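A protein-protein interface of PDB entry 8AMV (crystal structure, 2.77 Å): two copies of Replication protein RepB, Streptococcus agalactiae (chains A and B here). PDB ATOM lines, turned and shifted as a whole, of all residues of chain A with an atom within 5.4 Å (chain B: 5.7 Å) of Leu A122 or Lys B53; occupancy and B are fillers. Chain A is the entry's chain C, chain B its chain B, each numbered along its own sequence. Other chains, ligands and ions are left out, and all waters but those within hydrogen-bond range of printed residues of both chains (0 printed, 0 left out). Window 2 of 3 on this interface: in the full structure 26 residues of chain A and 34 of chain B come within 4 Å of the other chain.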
ATOM      1  N   MET A  33     -18.677  22.989 -15.343  1.00  0.00           N
ATOM      2  CA  MET A  33     -20.048  23.088 -14.882  1.00  0.00           C
ATOM      3  C   MET A  33     -20.972  23.033 -16.082  1.00  0.00           C
ATOM      4  O   MET A  33     -20.632  23.508 -17.168  1.00  0.00           O
ATOM      5  CB  MET A  33     -20.334  24.388 -14.098  1.00  0.00           C
ATOM      6  CG  MET A  33     -19.624  24.522 -12.755  1.00  0.00           C
ATOM      7  SD  MET A  33     -20.058  26.112 -12.028  1.00  0.00           S
ATOM      8  CE  MET A  33     -18.722  26.401 -10.855  1.00  0.00           C
ATOM      9  N   ALA A  34     -22.136  22.420 -15.883  1.00  0.00           N
ATOM     10  CA  ALA A  34     -23.230  22.448 -16.846  1.00  0.00           C
ATOM     11  C   ALA A  34     -24.385  23.213 -16.207  1.00  0.00           C
ATOM     12  O   ALA A  34     -24.808  22.881 -15.093  1.00  0.00           O
ATOM     13  CB  ALA A  34     -23.665  21.038 -17.246  1.00  0.00           C
ATOM     14  N   ILE A  35     -24.885  24.234 -16.908  1.00  0.00           N
ATOM     15  CA  ILE A  35     -25.996  25.062 -16.440  1.00  0.00           C
ATOM     16  C   ILE A  35     -27.212  24.649 -17.250  1.00  0.00           C
ATOM     17  O   ILE A  35     -27.207  24.764 -18.481  1.00  0.00           O
ATOM     18  CB  ILE A  35     -25.720  26.562 -16.651  1.00  0.00           C
ATOM     19  CG1 ILE A  35     -24.403  27.010 -16.025  1.00  0.00           C
ATOM     20  CG2 ILE A  35     -26.871  27.383 -16.106  1.00  0.00           C
ATOM     21  CD1 ILE A  35     -24.209  26.568 -14.600  1.00  0.00           C
ATOM     22  N   TYR A  97     -27.218  14.888 -15.694  1.00  0.00           N
ATOM     23  CA  TYR A  97     -27.047  15.728 -16.876  1.00  0.00           C
ATOM     24  C   TYR A  97     -28.316  15.725 -17.724  1.00  0.00           C
ATOM     25  O   TYR A  97     -28.708  16.754 -18.285  1.00  0.00           O
ATOM     26  CB  TYR A  97     -25.851  15.236 -17.707  1.00  0.00           C
ATOM     27  CG  TYR A  97     -25.552  16.096 -18.923  1.00  0.00           C
ATOM     28  CD1 TYR A  97     -26.303  15.977 -20.089  1.00  0.00           C
ATOM     29  CD2 TYR A  97     -24.530  17.043 -18.898  1.00  0.00           C
ATOM     30  CE1 TYR A  97     -26.053  16.773 -21.177  1.00  0.00           C
ATOM     31  CE2 TYR A  97     -24.271  17.841 -19.991  1.00  0.00           C
ATOM     32  CZ  TYR A  97     -25.036  17.698 -21.121  1.00  0.00           C
ATOM     33  OH  TYR A  97     -24.784  18.486 -22.209  1.00  0.00           O
ATOM     34  N   ILE A 120     -28.522  24.551 -22.609  1.00  0.00           N
ATOM     35  CA  ILE A 120     -27.466  24.111 -21.704  1.00  0.00           C
ATOM     36  C   ILE A 120     -26.206  24.895 -22.029  1.00  0.00           C
ATOM     37  O   ILE A 120     -25.709  24.842 -23.156  1.00  0.00           O
ATOM     38  CB  ILE A 120     -27.205  22.597 -21.802  1.00  0.00           C
ATOM     39  CG1 ILE A 120     -28.449  21.783 -21.454  1.00  0.00           C
ATOM     40  CG2 ILE A 120     -26.114  22.205 -20.859  1.00  0.00           C
ATOM     41  CD1 ILE A 120     -28.240  20.256 -21.531  1.00  0.00           C
ATOM     42  N   LYS A 121     -25.668  25.607 -21.048  1.00  0.00           N
ATOM     43  CA  LYS A 121     -24.392  26.285 -21.210  1.00  0.00           C
ATOM     44  C   LYS A 121     -23.323  25.479 -20.498  1.00  0.00           C
ATOM     45  O   LYS A 121     -23.447  25.193 -19.305  1.00  0.00           O
ATOM     46  CB  LYS A 121     -24.431  27.719 -20.679  1.00  0.00           C
ATOM     47  CG  LYS A 121     -25.210  28.697 -21.565  1.00  0.00           C
ATOM     48  CD  LYS A 121     -25.044  30.156 -21.105  1.00  0.00           C
ATOM     49  CE  LYS A 121     -26.327  30.701 -20.453  1.00  0.00           C
ATOM     50  NZ  LYS A 121     -26.389  32.187 -20.408  1.00  0.00           N
ATOM     51  N   LEU A 122     -22.277  25.115 -21.228  1.00  0.00           N
ATOM     52  CA  LEU A 122     -21.162  24.412 -20.621  1.00  0.00           C
ATOM     53  C   LEU A 122     -20.065  25.411 -20.302  1.00  0.00           C
ATOM     54  O   LEU A 122     -19.844  26.381 -21.030  1.00  0.00           O
ATOM     55  CB  LEU A 122     -20.637  23.290 -21.523  1.00  0.00           C
ATOM     56  CG  LEU A 122     -21.705  22.410 -22.180  1.00  0.00           C
ATOM     57  CD1 LEU A 122     -21.048  21.281 -22.958  1.00  0.00           C
ATOM     58  CD2 LEU A 122     -22.667  21.858 -21.147  1.00  0.00           C
ATOM     59  N   ILE A 123     -19.394  25.178 -19.187  1.00  0.00           N
ATOM     60  CA  ILE A 123     -18.423  26.126 -18.668  1.00  0.00           C
ATOM     61  C   ILE A 123     -17.129  25.392 -18.345  1.00  0.00           C
ATOM     62  O   ILE A 123     -17.147  24.296 -17.774  1.00  0.00           O
ATOM     63  CB  ILE A 123     -18.999  26.854 -17.432  1.00  0.00           C
ATOM     64  CG1 ILE A 123     -19.977  27.947 -17.877  1.00  0.00           C
ATOM     65  CG2 ILE A 123     -17.903  27.426 -16.520  1.00  0.00           C
ATOM     66  CD1 ILE A 123     -20.707  28.606 -16.726  1.00  0.00           C
ATOM     67  N   ASN A 124     -16.003  26.019 -18.690  1.00  0.00           N
ATOM     68  CA  ASN A 124     -14.667  25.551 -18.307  1.00  0.00           C
ATOM     69  C   ASN A 124     -14.397  24.123 -18.787  1.00  0.00           C
ATOM     70  O   ASN A 124     -13.977  23.258 -18.023  1.00  0.00           O
ATOM     71  CB  ASN A 124     -14.474  25.692 -16.791  1.00  0.00           C
ATOM     72  CG  ASN A 124     -14.544  27.135 -16.344  1.00  0.00           C
ATOM     73  OD1 ASN A 124     -14.593  28.040 -17.174  1.00  0.00           O
ATOM     74  ND2 ASN A 124     -14.556  27.364 -15.037  1.00  0.00           N
ATOM     75  N   ASN A 125     -14.644  23.898 -20.084  1.00  0.00           N
ATOM     76  CA  ASN A 125     -14.325  22.625 -20.740  1.00  0.00           C
ATOM     77  C   ASN A 125     -15.039  21.457 -20.084  1.00  0.00           C
ATOM     78  O   ASN A 125     -14.468  20.385 -19.879  1.00  0.00           O
ATOM     79  CB  ASN A 125     -12.819  22.368 -20.753  1.00  0.00           C
ATOM     80  CG  ASN A 125     -12.069  23.509 -21.334  1.00  0.00           C
ATOM     81  OD1 ASN A 125     -12.354  23.909 -22.452  1.00  0.00           O
ATOM     82  ND2 ASN A 125     -11.107  24.051 -20.588  1.00  0.00           N
ATOM     83  N   PHE A 126     -16.292  21.680 -19.735  1.00  0.00           N
ATOM     84  CA  PHE A 126     -17.132  20.600 -19.256  1.00  0.00           C
ATOM     85  C   PHE A 126     -17.342  19.639 -20.413  1.00  0.00           C
ATOM     86  O   PHE A 126     -17.968  19.997 -21.412  1.00  0.00           O
ATOM     87  CB  PHE A 126     -18.458  21.161 -18.746  1.00  0.00           C
ATOM     88  CG  PHE A 126     -19.358  20.143 -18.086  1.00  0.00           C
ATOM     89  CD1 PHE A 126     -20.146  19.274 -18.840  1.00  0.00           C
ATOM     90  CD2 PHE A 126     -19.432  20.077 -16.707  1.00  0.00           C
ATOM     91  CE1 PHE A 126     -20.965  18.357 -18.220  1.00  0.00           C
ATOM     92  CE2 PHE A 126     -20.244  19.171 -16.090  1.00  0.00           C
ATOM     93  CZ  PHE A 126     -21.016  18.308 -16.845  1.00  0.00           C
ATOM     94  N   ASP A 127     -16.852  18.411 -20.271  1.00  0.00           N
ATOM     95  CA  ASP A 127     -17.007  17.366 -21.280  1.00  0.00           C
ATOM     96  C   ASP A 127     -17.638  16.192 -20.556  1.00  0.00           C
ATOM     97  O   ASP A 127     -16.955  15.484 -19.815  1.00  0.00           O
ATOM     98  CB  ASP A 127     -15.649  17.003 -21.895  1.00  0.00           C
ATOM     99  CG  ASP A 127     -15.738  15.889 -22.934  1.00  0.00           C
ATOM    100  OD1 ASP A 127     -16.865  15.459 -23.277  1.00  0.00           O
ATOM    101  OD2 ASP A 127     -14.658  15.429 -23.391  1.00  0.00           O
ATOM    102  N   ASP A 129     -18.502  13.293 -21.360  1.00  0.00           N
ATOM    103  CA  ASP A 129     -17.979  11.954 -21.621  1.00  0.00           C
ATOM    104  C   ASP A 129     -16.771  11.610 -20.747  1.00  0.00           C
ATOM    105  O   ASP A 129     -16.498  10.425 -20.522  1.00  0.00           O
ATOM    106  CB  ASP A 129     -17.617  11.812 -23.088  1.00  0.00           C
ATOM    107  CG  ASP A 129     -18.838  11.764 -23.965  1.00  0.00           C
ATOM    108  OD1 ASP A 129     -19.691  10.894 -23.718  1.00  0.00           O
ATOM    109  OD2 ASP A 129     -18.958  12.595 -24.887  1.00  0.00           O
ATOM    110  N   TYR B  14      -9.405  21.267 -26.069  1.00  0.00           N
ATOM    111  CA  TYR B  14     -10.594  21.322 -26.929  1.00  0.00           C
ATOM    112  C   TYR B  14     -10.538  22.564 -27.815  1.00  0.00           C
ATOM    113  O   TYR B  14     -10.121  23.626 -27.336  1.00  0.00           O
ATOM    114  CB  TYR B  14     -11.900  21.351 -26.128  1.00  0.00           C
ATOM    115  CG  TYR B  14     -11.990  20.308 -25.065  1.00  0.00           C
ATOM    116  CD1 TYR B  14     -11.365  20.486 -23.833  1.00  0.00           C
ATOM    117  CD2 TYR B  14     -12.697  19.143 -25.289  1.00  0.00           C
ATOM    118  CE1 TYR B  14     -11.443  19.521 -22.849  1.00  0.00           C
ATOM    119  CE2 TYR B  14     -12.782  18.172 -24.318  1.00  0.00           C
ATOM    120  CZ  TYR B  14     -12.155  18.364 -23.104  1.00  0.00           C
ATOM    121  OH  TYR B  14     -12.245  17.393 -22.145  1.00  0.00           O
ATOM    122  N   GLU B  16     -12.779  24.685 -28.811  1.00  0.00           N
ATOM    123  CA  GLU B  16     -13.555  25.793 -28.238  1.00  0.00           C
ATOM    124  C   GLU B  16     -12.811  26.558 -27.148  1.00  0.00           C
ATOM    125  O   GLU B  16     -13.295  27.595 -26.692  1.00  0.00           O
ATOM    126  CB  GLU B  16     -14.896  25.342 -27.629  1.00  0.00           C
ATOM    127  CG  GLU B  16     -14.817  24.264 -26.553  1.00  0.00           C
ATOM    128  CD  GLU B  16     -16.137  23.533 -26.348  1.00  0.00           C
ATOM    129  OE1 GLU B  16     -17.086  23.800 -27.124  1.00  0.00           O
ATOM    130  OE2 GLU B  16     -16.233  22.717 -25.399  1.00  0.00           O
ATOM    131  N   HIS B  39      -9.704  14.426 -32.350  1.00  0.00           N
ATOM    132  CA  HIS B  39     -10.621  13.303 -32.160  1.00  0.00           C
ATOM    133  C   HIS B  39     -12.050  13.825 -32.306  1.00  0.00           C
ATOM    134  O   HIS B  39     -12.788  13.989 -31.333  1.00  0.00           O
ATOM    135  CB  HIS B  39     -10.423  12.667 -30.786  1.00  0.00           C
ATOM    136  CG  HIS B  39      -9.154  11.886 -30.640  1.00  0.00           C
ATOM    137  ND1 HIS B  39      -8.632  11.536 -29.414  1.00  0.00           N
ATOM    138  CD2 HIS B  39      -8.302  11.388 -31.566  1.00  0.00           C
ATOM    139  CE1 HIS B  39      -7.522  10.842 -29.590  1.00  0.00           C
ATOM    140  NE2 HIS B  39      -7.302  10.734 -30.888  1.00  0.00           N
ATOM    141  N   ASP B  42     -14.788  10.476 -32.134  1.00  0.00           N
ATOM    142  CA  ASP B  42     -14.737   9.560 -31.016  1.00  0.00           C
ATOM    143  C   ASP B  42     -16.167   9.201 -30.664  1.00  0.00           C
ATOM    144  O   ASP B  42     -16.971  10.075 -30.342  1.00  0.00           O
ATOM    145  CB  ASP B  42     -14.039  10.227 -29.830  1.00  0.00           C
ATOM    146  CG  ASP B  42     -12.567   9.900 -29.769  1.00  0.00           C
ATOM    147  OD1 ASP B  42     -12.057   9.230 -30.684  1.00  0.00           O
ATOM    148  OD2 ASP B  42     -11.908  10.343 -28.808  1.00  0.00           O
ATOM    149  N   GLN B  49     -25.491  12.171 -28.107  1.00  0.00           N
ATOM    150  CA  GLN B  49     -24.519  13.110 -28.645  1.00  0.00           C
ATOM    151  C   GLN B  49     -23.565  12.408 -29.618  1.00  0.00           C
ATOM    152  O   GLN B  49     -22.521  12.968 -29.957  1.00  0.00           O
ATOM    153  CB  GLN B  49     -23.887  13.861 -27.434  1.00  0.00           C
ATOM    154  CG  GLN B  49     -22.889  15.110 -27.517  1.00  0.00           C
ATOM    155  CD  GLN B  49     -21.954  15.232 -26.296  1.00  0.00           C
ATOM    156  OE1 GLN B  49     -22.360  14.879 -25.194  1.00  0.00           O
ATOM    157  NE2 GLN B  49     -20.735  15.712 -26.486  1.00  0.00           N
ATOM    158  N   TYR B  51     -21.046  11.435 -30.964  1.00  0.00           N
ATOM    159  CA  TYR B  51     -19.596  11.500 -30.849  1.00  0.00           C
ATOM    160  C   TYR B  51     -19.234  12.314 -29.610  1.00  0.00           C
ATOM    161  O   TYR B  51     -19.908  13.296 -29.281  1.00  0.00           O
ATOM    162  CB  TYR B  51     -18.966  12.169 -32.083  1.00  0.00           C
ATOM    163  CG  TYR B  51     -19.097  11.456 -33.436  1.00  0.00           C
ATOM    164  CD1 TYR B  51     -18.572  10.174 -33.652  1.00  0.00           C
ATOM    165  CD2 TYR B  51     -19.695  12.099 -34.515  1.00  0.00           C
ATOM    166  CE1 TYR B  51     -18.676   9.549 -34.913  1.00  0.00           C
ATOM    167  CE2 TYR B  51     -19.809  11.489 -35.771  1.00  0.00           C
ATOM    168  CZ  TYR B  51     -19.295  10.212 -35.972  1.00  0.00           C
ATOM    169  OH  TYR B  51     -19.405   9.612 -37.220  1.00  0.00           O
ATOM    170  N   LYS B  52     -18.128  11.953 -28.960  1.00  0.00           N
ATOM    171  CA  LYS B  52     -17.679  12.714 -27.800  1.00  0.00           C
ATOM    172  C   LYS B  52     -17.188  14.087 -28.237  1.00  0.00           C
ATOM    173  O   LYS B  52     -16.981  14.368 -29.426  1.00  0.00           O
ATOM    174  CB  LYS B  52     -16.554  12.005 -27.039  1.00  0.00           C
ATOM    175  CG  LYS B  52     -16.851  10.564 -26.675  1.00  0.00           C
ATOM    176  CD  LYS B  52     -15.602   9.652 -26.658  1.00  0.00           C
ATOM    177  CE  LYS B  52     -15.775   8.413 -25.788  1.00  0.00           C
ATOM    178  NZ  LYS B  52     -15.643   8.521 -24.342  1.00  0.00           N
ATOM    179  N   LYS B  53     -17.017  14.957 -27.249  1.00  0.00           N
ATOM    180  CA  LYS B  53     -16.517  16.290 -27.531  1.00  0.00           C
ATOM    181  C   LYS B  53     -15.203  16.186 -28.303  1.00  0.00           C
ATOM    182  O   LYS B  53     -14.293  15.441 -27.921  1.00  0.00           O
ATOM    183  CB  LYS B  53     -16.294  17.034 -26.213  1.00  0.00           C
ATOM    184  CG  LYS B  53     -17.413  17.929 -25.773  1.00  0.00           C
ATOM    185  CD  LYS B  53     -16.835  19.244 -25.282  1.00  0.00           C
ATOM    186  CE  LYS B  53     -17.795  19.968 -24.359  1.00  0.00           C
ATOM    187  NZ  LYS B  53     -17.376  21.374 -24.044  1.00  0.00           N
ATOM    188  N   ALA B  54     -15.130  16.887 -29.431  1.00  0.00           N
ATOM    189  CA  ALA B  54     -13.898  16.906 -30.202  1.00  0.00           C
ATOM    190  C   ALA B  54     -12.799  17.485 -29.324  1.00  0.00           C
ATOM    191  O   ALA B  54     -12.985  18.536 -28.700  1.00  0.00           O
ATOM    192  CB  ALA B  54     -14.073  17.730 -31.482  1.00  0.00           C
ATOM    193  N   HIS B  55     -11.658  16.801 -29.261  1.00  0.00           N
ATOM    194  CA  HIS B  55     -10.581  17.202 -28.361  1.00  0.00           C
ATOM    195  C   HIS B  55      -9.224  16.775 -28.920  1.00  0.00           C
ATOM    196  O   HIS B  55      -9.136  16.013 -29.887  1.00  0.00           O
ATOM    197  CB  HIS B  55     -10.800  16.598 -26.968  1.00  0.00           C
ATOM    198  CG  HIS B  55     -10.740  15.106 -26.957  1.00  0.00           C
ATOM    199  ND1 HIS B  55     -11.686  14.315 -27.578  1.00  0.00           N
ATOM    200  CD2 HIS B  55      -9.821  14.259 -26.436  1.00  0.00           C
ATOM    201  CE1 HIS B  55     -11.365  13.045 -27.410  1.00  0.00           C
ATOM    202  NE2 HIS B  55     -10.238  12.983 -26.721  1.00  0.00           N
ATOM    203  N   LYS B  82      -8.864  29.502 -19.627  1.00  0.00           N
ATOM    204  CA  LYS B  82     -10.001  28.660 -19.926  1.00  0.00           C
ATOM    205  C   LYS B  82      -9.584  27.481 -20.819  1.00  0.00           C
ATOM    206  O   LYS B  82     -10.441  26.815 -21.402  1.00  0.00           O
ATOM    207  CB  LYS B  82     -11.117  29.495 -20.539  1.00  0.00           C
ATOM    208  CG  LYS B  82     -12.523  29.059 -20.156  1.00  0.00           C
ATOM    209  CD  LYS B  82     -13.119  28.242 -21.287  1.00  0.00           C
ATOM    210  CE  LYS B  82     -14.542  27.813 -21.022  1.00  0.00           C
ATOM    211  NZ  LYS B  82     -14.854  26.486 -21.650  1.00  0.00           N
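CD1 of Leu A122 touches CE of Lys B53, at 3.8 Å. Asn A125 touches Tyr B14. Asp A127 touches Lys B53. Asp A129 touches Gln B49. Lys B52 touches Asp A129. Asp A129 touches Lys B53.
Printed residues of chain A that touch a printed residue of chain B: Leu A122, Asn A124, Asn A125, Phe A126, Asp A127 and Asp A129. Hydrophobic or aromatic side chains of chain A that line the printed part of chain B: Leu A122. Of the 11 printed residues of chain B, 5 touch a printed residue of chain A. Printed residues of chain B that touch a printed residue of chain A: Tyr B14, Gln B49, Lys B52, Lys B53 and Lys B82. Among the printed residues, no Asp or Glu carboxylate lies within 4 Å of a Lys or Arg side-chain nitrogen of the other chain.
Of the printed residues of chain B, Phe A126 touches Lys B53 (3.0 Å). Of the printed residues of chain B, Asp A129 touches Gln B49, Lys B52 and Lys B53. Printed residues of chain B within 4 Å of Asn A124: Lys B82. Glu B16 touches none of the printed residues of chain A. The nearest printed residue of chain B that does not touch Asp A127 is Gln B49 (5.0 Å).
The side-chain amino group of Lys B82 lies close to the backbone NH of Asn A124, 3.2 Å away. The backbone carbonyl oxygen (O) of Lys B82 sits at hydrogen-bond distance from the side-chain amide nitrogen (ND2) of Asn A125 (3.0 Å). OH of Tyr B14 is in hydrogen-bond range of OD2 of Asp A127 (3.4 Å). The backbone carbonyl oxygen (O) of Phe A126 lies close to the side-chain amino group (NZ) of Lys B53.
No position is printed for both chains.
OD1 of Asp A127 sits close to N of Asp A129 (3.3 Å). NZ of Lys B53 is in salt-bridge range of OE1 of Glu B16 (3.9 Å). The backbone NH (N) of Lys B52 sits at hydrogen-bond distance from the backbone carbonyl oxygen (O) of Asp B42, 2.6 Å away. ND1 of His B55 sits at hydrogen-bond distance from O of Lys B53.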
